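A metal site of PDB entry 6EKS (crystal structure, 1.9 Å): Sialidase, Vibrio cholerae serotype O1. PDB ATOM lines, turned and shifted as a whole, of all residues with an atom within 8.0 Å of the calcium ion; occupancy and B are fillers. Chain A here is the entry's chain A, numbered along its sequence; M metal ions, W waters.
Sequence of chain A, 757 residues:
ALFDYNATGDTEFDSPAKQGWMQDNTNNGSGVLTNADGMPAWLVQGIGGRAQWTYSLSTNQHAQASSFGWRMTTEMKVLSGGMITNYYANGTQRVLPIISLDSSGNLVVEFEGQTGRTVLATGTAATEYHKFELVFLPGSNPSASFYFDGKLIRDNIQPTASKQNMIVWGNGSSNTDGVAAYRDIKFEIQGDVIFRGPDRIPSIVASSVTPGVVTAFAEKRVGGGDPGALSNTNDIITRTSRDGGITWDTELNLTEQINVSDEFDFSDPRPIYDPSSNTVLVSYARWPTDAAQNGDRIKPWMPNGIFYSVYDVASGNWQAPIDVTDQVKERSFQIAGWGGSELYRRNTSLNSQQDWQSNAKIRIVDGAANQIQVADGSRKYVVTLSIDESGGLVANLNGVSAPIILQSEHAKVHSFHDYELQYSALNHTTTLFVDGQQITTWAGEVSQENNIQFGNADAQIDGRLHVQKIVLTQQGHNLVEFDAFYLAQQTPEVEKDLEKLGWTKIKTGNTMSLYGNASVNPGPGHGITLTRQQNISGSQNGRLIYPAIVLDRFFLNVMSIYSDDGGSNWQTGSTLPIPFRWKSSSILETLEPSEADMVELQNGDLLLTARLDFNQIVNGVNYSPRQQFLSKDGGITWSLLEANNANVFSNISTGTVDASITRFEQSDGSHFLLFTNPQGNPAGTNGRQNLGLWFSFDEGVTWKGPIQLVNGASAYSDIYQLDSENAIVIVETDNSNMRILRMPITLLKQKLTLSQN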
ATOM      1  N   ILE A 201     -17.769  25.906  15.740  1.00  0.00           N
ATOM      2  CA  ILE A 201     -16.733  26.839  15.272  1.00  0.00           C
ATOM      3  C   ILE A 201     -16.330  27.854  16.348  1.00  0.00           C
ATOM      4  O   ILE A 201     -16.610  29.062  16.236  1.00  0.00           O
ATOM      5  CB  ILE A 201     -17.173  27.608  13.993  1.00  0.00           C
ATOM      6  CG1 ILE A 201     -17.914  26.693  13.007  1.00  0.00           C
ATOM      7  CG2 ILE A 201     -15.928  28.180  13.289  1.00  0.00           C
ATOM      8  CD1 ILE A 201     -17.175  25.364  12.739  1.00  0.00           C
ATOM      9  N   PRO A 202     -15.639  27.373  17.392  1.00  0.00           N
ATOM     10  CA  PRO A 202     -15.356  28.189  18.570  1.00  0.00           C
ATOM     11  C   PRO A 202     -14.115  29.042  18.457  1.00  0.00           C
ATOM     12  O   PRO A 202     -13.165  28.697  17.743  1.00  0.00           O
ATOM     13  CB  PRO A 202     -15.162  27.126  19.676  1.00  0.00           C
ATOM     14  CG  PRO A 202     -14.528  25.963  18.917  1.00  0.00           C
ATOM     15  CD  PRO A 202     -15.160  25.981  17.537  1.00  0.00           C
ATOM     16  N   SER A 203     -14.116  30.165  19.173  1.00  0.00           N
ATOM     17  CA  SER A 203     -12.936  30.979  19.336  1.00  0.00           C
ATOM     18  C   SER A 203     -12.966  31.608  20.732  1.00  0.00           C
ATOM     19  O   SER A 203     -14.021  31.721  21.362  1.00  0.00           O
ATOM     20  CB  SER A 203     -12.852  32.061  18.243  1.00  0.00           C
ATOM     21  OG  SER A 203     -14.011  32.880  18.276  1.00  0.00           O
ATOM     22  N   ARG A 270     -14.139  35.697  14.580  1.00  0.00           N
ATOM     23  CA  ARG A 270     -12.700  35.891  14.708  1.00  0.00           C
ATOM     24  C   ARG A 270     -12.381  37.099  15.615  1.00  0.00           C
ATOM     25  O   ARG A 270     -12.289  38.258  15.150  1.00  0.00           O
ATOM     26  CB  ARG A 270     -12.078  36.077  13.302  1.00  0.00           C
ATOM     27  CG  ARG A 270     -10.599  36.419  13.298  1.00  0.00           C
ATOM     28  CD  ARG A 270      -9.743  35.195  13.463  1.00  0.00           C
ATOM     29  NE  ARG A 270      -9.713  34.414  12.222  1.00  0.00           N
ATOM     30  CZ  ARG A 270      -8.920  33.371  12.028  1.00  0.00           C
ATOM     31  NH1 ARG A 270      -8.109  32.984  13.003  1.00  0.00           N
ATOM     32  NH2 ARG A 270      -8.950  32.710  10.848  1.00  0.00           N
ATOM     33  N   GLY A 523     -12.598  33.425   8.896  1.00  0.00           N
ATOM     34  CA  GLY A 523     -12.067  32.111   9.244  1.00  0.00           C
ATOM     35  C   GLY A 523     -12.131  31.862  10.763  1.00  0.00           C
ATOM     36  O   GLY A 523     -12.362  32.788  11.533  1.00  0.00           O
ATOM     37  N   PRO A 524     -11.924  30.609  11.180  1.00  0.00           N
ATOM     38  CA  PRO A 524     -12.121  30.194  12.591  1.00  0.00           C
ATOM     39  C   PRO A 524     -10.909  30.364  13.510  1.00  0.00           C
ATOM     40  O   PRO A 524      -9.789  29.913  13.226  1.00  0.00           O
ATOM     41  CB  PRO A 524     -12.460  28.707  12.458  1.00  0.00           C
ATOM     42  CG  PRO A 524     -11.639  28.242  11.264  1.00  0.00           C
ATOM     43  CD  PRO A 524     -11.610  29.469  10.292  1.00  0.00           C
ATOM     44  N   GLY A 525     -11.164  30.968  14.666  1.00  0.00           N
ATOM     45  CA  GLY A 525     -10.120  31.169  15.657  1.00  0.00           C
ATOM     46  C   GLY A 525     -10.082  32.636  16.046  1.00  0.00           C
ATOM     47  O   GLY A 525     -11.077  33.345  15.954  1.00  0.00           O
ATOM     48  N   HIS A 526      -8.922  33.097  16.482  1.00  0.00           N
ATOM     49  CA  HIS A 526      -8.813  34.507  16.839  1.00  0.00           C
ATOM     50  C   HIS A 526      -7.696  35.148  16.053  1.00  0.00           C
ATOM     51  O   HIS A 526      -6.941  34.467  15.345  1.00  0.00           O
ATOM     52  CB  HIS A 526      -8.577  34.662  18.347  1.00  0.00           C
ATOM     53  CG  HIS A 526      -7.345  33.993  18.831  1.00  0.00           C
ATOM     54  ND1 HIS A 526      -7.357  32.722  19.374  1.00  0.00           N
ATOM     55  CD2 HIS A 526      -6.047  34.399  18.833  1.00  0.00           C
ATOM     56  CE1 HIS A 526      -6.114  32.373  19.700  1.00  0.00           C
ATOM     57  NE2 HIS A 526      -5.312  33.369  19.379  1.00  0.00           N
ATOM     58  N   PRO A 547      -5.911  36.180   9.723  1.00  0.00           N
ATOM     59  CA  PRO A 547      -5.764  35.532   8.423  1.00  0.00           C
ATOM     60  C   PRO A 547      -7.108  35.064   7.878  1.00  0.00           C
ATOM     61  O   PRO A 547      -7.646  34.072   8.342  1.00  0.00           O
ATOM     62  CB  PRO A 547      -4.838  34.364   8.712  1.00  0.00           C
ATOM     63  CG  PRO A 547      -5.174  33.964  10.160  1.00  0.00           C
ATOM     64  CD  PRO A 547      -5.758  35.227  10.836  1.00  0.00           C
ATOM     65  N   GLU A 595      -8.533  27.523   6.438  1.00  0.00           N
ATOM     66  CA  GLU A 595      -8.649  27.911   7.843  1.00  0.00           C
ATOM     67  C   GLU A 595      -7.280  28.085   8.472  1.00  0.00           C
ATOM     68  O   GLU A 595      -6.501  27.149   8.569  1.00  0.00           O
ATOM     69  CB  GLU A 595      -9.486  26.865   8.605  1.00  0.00           C
ATOM     70  CG  GLU A 595     -10.920  26.839   8.087  1.00  0.00           C
ATOM     71  CD  GLU A 595     -11.782  25.760   8.724  1.00  0.00           C
ATOM     72  OE1 GLU A 595     -11.215  24.804   9.270  1.00  0.00           O
ATOM     73  OE2 GLU A 595     -13.028  25.893   8.659  1.00  0.00           O
ATOM     74  N   ALA A 596      -6.987  29.291   8.939  1.00  0.00           N
ATOM     75  CA  ALA A 596      -5.621  29.594   9.313  1.00  0.00           C
ATOM     76  C   ALA A 596      -5.536  30.394  10.598  1.00  0.00           C
ATOM     77  O   ALA A 596      -6.494  31.007  11.023  1.00  0.00           O
ATOM     78  CB  ALA A 596      -4.927  30.347   8.166  1.00  0.00           C
ATOM     79  N   ASP A 597      -4.358  30.368  11.199  1.00  0.00           N
ATOM     80  CA  ASP A 597      -4.117  31.022  12.485  1.00  0.00           C
ATOM     81  C   ASP A 597      -2.687  31.534  12.474  1.00  0.00           C
ATOM     82  O   ASP A 597      -1.791  30.856  11.954  1.00  0.00           O
ATOM     83  CB  ASP A 597      -4.377  30.037  13.646  1.00  0.00           C
ATOM     84  CG  ASP A 597      -5.797  29.467  13.630  1.00  0.00           C
ATOM     85  OD1 ASP A 597      -6.075  28.490  12.886  1.00  0.00           O
ATOM     86  OD2 ASP A 597      -6.661  30.006  14.353  1.00  0.00           O
ATOM     87  N   MET A 598      -2.450  32.718  13.015  1.00  0.00           N
ATOM     88  CA  MET A 598      -1.107  33.255  12.974  1.00  0.00           C
ATOM     89  C   MET A 598      -0.650  33.714  14.354  1.00  0.00           C
ATOM     90  O   MET A 598      -1.460  34.004  15.238  1.00  0.00           O
ATOM     91  CB  MET A 598      -1.018  34.420  11.958  1.00  0.00           C
ATOM     92  CG  MET A 598      -1.741  35.688  12.418  1.00  0.00           C
ATOM     93  SD  MET A 598      -1.386  37.184  11.440  1.00  0.00           S
ATOM     94  CE  MET A 598      -2.257  36.789   9.927  1.00  0.00           C
ATOM     95  N   THR A 609      -0.155  29.170  10.226  1.00  0.00           N
ATOM     96  CA  THR A 609      -0.410  27.750   9.992  1.00  0.00           C
ATOM     97  C   THR A 609      -1.791  27.620   9.365  1.00  0.00           C
ATOM     98  O   THR A 609      -2.772  28.173   9.896  1.00  0.00           O
ATOM     99  CB  THR A 609      -0.309  26.908  11.301  1.00  0.00           C
ATOM    100  OG1 THR A 609      -0.575  25.533  10.995  1.00  0.00           O
ATOM    101  CG2 THR A 609      -1.276  27.407  12.401  1.00  0.00           C
ATOM    102  N   ARG A 626      -1.721  20.350   6.297  1.00  0.00           N
ATOM    103  CA  ARG A 626      -1.431  21.609   6.977  1.00  0.00           C
ATOM    104  C   ARG A 626      -0.090  22.162   6.493  1.00  0.00           C
ATOM    105  O   ARG A 626       0.818  21.401   6.241  1.00  0.00           O
ATOM    106  CB  ARG A 626      -1.425  21.412   8.494  1.00  0.00           C
ATOM    107  CG  ARG A 626      -1.126  22.671   9.310  1.00  0.00           C
ATOM    108  CD  ARG A 626      -1.648  22.470  10.740  1.00  0.00           C
ATOM    109  NE  ARG A 626      -3.115  22.460  10.725  1.00  0.00           N
ATOM    110  CZ  ARG A 626      -3.865  23.559  10.739  1.00  0.00           C
ATOM    111  NH1 ARG A 626      -3.290  24.777  10.811  1.00  0.00           N
ATOM    112  NH2 ARG A 626      -5.177  23.451  10.706  1.00  0.00           N
ATOM    113  N   VAL A 657      -8.613  19.773   9.391  1.00  0.00           N
ATOM    114  CA  VAL A 657      -9.380  20.308  10.494  1.00  0.00           C
ATOM    115  C   VAL A 657      -8.777  21.642  10.872  1.00  0.00           C
ATOM    116  O   VAL A 657      -7.593  21.863  10.637  1.00  0.00           O
ATOM    117  CB  VAL A 657      -9.364  19.333  11.696  1.00  0.00           C
ATOM    118  CG1 VAL A 657      -7.964  19.182  12.224  1.00  0.00           C
ATOM    119  CG2 VAL A 657     -10.329  19.789  12.795  1.00  0.00           C
ATOM    120  N   ASP A 658      -9.571  22.539  11.450  1.00  0.00           N
ATOM    121  CA  ASP A 658      -9.030  23.772  12.025  1.00  0.00           C
ATOM    122  C   ASP A 658      -8.129  23.493  13.223  1.00  0.00           C
ATOM    123  O   ASP A 658      -8.396  22.563  14.024  1.00  0.00           O
ATOM    124  CB  ASP A 658     -10.139  24.717  12.461  1.00  0.00           C
ATOM    125  CG  ASP A 658      -9.599  26.043  12.937  1.00  0.00           C
ATOM    126  OD1 ASP A 658      -8.743  26.605  12.226  1.00  0.00           O
ATOM    127  OD2 ASP A 658     -10.004  26.503  14.032  1.00  0.00           O
ATOM    128  N   ALA A 659      -7.083  24.302  13.345  1.00  0.00           N
ATOM    129  CA  ALA A 659      -6.163  24.229  14.478  1.00  0.00           C
ATOM    130  C   ALA A 659      -6.141  25.583  15.220  1.00  0.00           C
ATOM    131  O   ALA A 659      -6.882  26.489  14.878  1.00  0.00           O
ATOM    132  CB  ALA A 659      -4.753  23.850  13.983  1.00  0.00           C
ATOM    133  N   SER A 660      -5.297  25.695  16.245  1.00  0.00           N
ATOM    134  CA  SER A 660      -5.085  26.969  16.924  1.00  0.00           C
ATOM    135  C   SER A 660      -3.616  27.115  17.228  1.00  0.00           C
ATOM    136  O   SER A 660      -2.921  26.115  17.416  1.00  0.00           O
ATOM    137  CB  SER A 660      -5.927  27.064  18.198  1.00  0.00           C
ATOM    138  OG  SER A 660      -5.914  28.402  18.716  1.00  0.00           O
ATOM    139  N   ILE A 661      -3.146  28.367  17.251  1.00  0.00           N
ATOM    140  CA  ILE A 661      -1.772  28.659  17.622  1.00  0.00           C
ATOM    141  C   ILE A 661      -1.729  29.964  18.445  1.00  0.00           C
ATOM    142  O   ILE A 661      -2.521  30.881  18.207  1.00  0.00           O
ATOM    143  CB  ILE A 661      -0.849  28.727  16.358  1.00  0.00           C
ATOM    144  CG1 ILE A 661       0.623  28.624  16.748  1.00  0.00           C
ATOM    145  CG2 ILE A 661      -1.154  29.975  15.485  1.00  0.00           C
ATOM    146  CD1 ILE A 661       1.589  28.547  15.549  1.00  0.00           C
ATOM    147  N   THR A 676      -2.829  23.578  19.157  1.00  0.00           N
ATOM    148  CA  THR A 676      -3.788  22.504  19.445  1.00  0.00           C
ATOM    149  C   THR A 676      -4.430  21.990  18.152  1.00  0.00           C
ATOM    150  O   THR A 676      -4.680  22.762  17.210  1.00  0.00           O
ATOM    151  CB  THR A 676      -4.927  22.947  20.414  1.00  0.00           C
ATOM    152  OG1 THR A 676      -5.549  24.153  19.915  1.00  0.00           O
ATOM    153  CG2 THR A 676      -4.377  23.196  21.833  1.00  0.00           C
ATOM    154  N   TYR A 716     -12.682  21.169  16.108  1.00  0.00           N
ATOM    155  CA  TYR A 716     -12.118  22.541  16.130  1.00  0.00           C
ATOM    156  C   TYR A 716     -11.754  22.942  17.549  1.00  0.00           C
ATOM    157  O   TYR A 716     -12.392  22.532  18.506  1.00  0.00           O
ATOM    158  CB  TYR A 716     -13.077  23.574  15.570  1.00  0.00           C
ATOM    159  CG  TYR A 716     -13.227  23.551  14.063  1.00  0.00           C
ATOM    160  CD1 TYR A 716     -13.075  22.371  13.341  1.00  0.00           C
ATOM    161  CD2 TYR A 716     -13.548  24.719  13.365  1.00  0.00           C
ATOM    162  CE1 TYR A 716     -13.227  22.340  11.936  1.00  0.00           C
ATOM    163  CE2 TYR A 716     -13.696  24.717  12.000  1.00  0.00           C
ATOM    164  CZ  TYR A 716     -13.546  23.522  11.294  1.00  0.00           C
ATOM    165  OH  TYR A 716     -13.701  23.538   9.945  1.00  0.00           O
ATOM    166  N   SER A 717     -10.718  23.750  17.680  1.00  0.00           N
ATOM    167  CA  SER A 717     -10.279  24.215  18.977  1.00  0.00           C
ATOM    168  C   SER A 717      -9.661  25.595  18.869  1.00  0.00           C
ATOM    169  O   SER A 717      -9.282  26.029  17.778  1.00  0.00           O
ATOM    170  CB  SER A 717      -9.269  23.236  19.577  1.00  0.00           C
ATOM    171  OG  SER A 717      -8.061  23.285  18.836  1.00  0.00           O
ATOM    172  N   ASP A 718      -9.575  26.282  19.998  1.00  0.00           N
ATOM    173  CA  ASP A 718      -8.869  27.549  20.072  1.00  0.00           C
ATOM    174  C   ASP A 718      -8.243  27.661  21.447  1.00  0.00           C
ATOM    175  O   ASP A 718      -8.848  27.265  22.441  1.00  0.00           O
ATOM    176  CB  ASP A 718      -9.804  28.727  19.794  1.00  0.00           C
ATOM    177  CG  ASP A 718      -9.060  29.940  19.241  1.00  0.00           C
ATOM    178  OD1 ASP A 718      -8.090  29.747  18.468  1.00  0.00           O
ATOM    179  OD2 ASP A 718      -9.439  31.082  19.593  1.00  0.00           O
ATOM    180  N   ILE A 719      -7.011  28.154  21.480  1.00  0.00           N
ATOM    181  CA  ILE A 719      -6.255  28.246  22.733  1.00  0.00           C
ATOM    182  C   ILE A 719      -5.762  29.686  22.926  1.00  0.00           C
ATOM    183  O   ILE A 719      -5.388  30.367  21.936  1.00  0.00           O
ATOM    184  CB  ILE A 719      -5.079  27.251  22.745  1.00  0.00           C
ATOM    185  CG1 ILE A 719      -4.381  27.258  24.106  1.00  0.00           C
ATOM    186  CG2 ILE A 719      -4.121  27.507  21.537  1.00  0.00           C
ATOM    187  CD1 ILE A 719      -3.503  26.048  24.350  1.00  0.00           C
HETATM  188 CA    CA M   1      -8.216  28.155  13.953  1.00  0.00          CA
HETATM  189  O   HOH W   1      -8.972  28.272  16.135  1.00  0.00           O
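The side-chain carboxylate (OD2) of Asp 597 sits close to the guanidinium group (NH1) of Arg 270 (3.6 Å). The backbone carbonyl oxygen (O) of Asp 597 is in hydrogen-bond range of the backbone NH (N) of Thr 609.
Gly 525 touches the calcium ion. The nearest printed residue that does not touch the calcium ion is Ala 596 (4.4 Å).
Water W1 is bound to the calcium ion (2.3 Å). The calcium ion is bound by O of Ala 659, 2.3 Å away. OD1 of Asp 658 is bound to the calcium ion (2.4 Å). The side-chain carboxylate (OD1) of Asp 597 is bound to the calcium ion (2.4 Å). OD2 of Asp 658 is bound to the calcium ion (2.4 Å). The side-chain carboxylate (OD2) of Asp 597 binds the calcium ion, at 2.5 Å. The backbone carbonyl oxygen (O) of Pro 524 binds the calcium ion, 2.5 Å away. The calcium ion has seven donor atoms within binding distance.
Water W1 lies within hydrogen-bond range of the backbone carbonyl oxygen of Ser 717 (2.8 Å) and the side-chain carboxylate of Asp 718 (2.9 Å).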
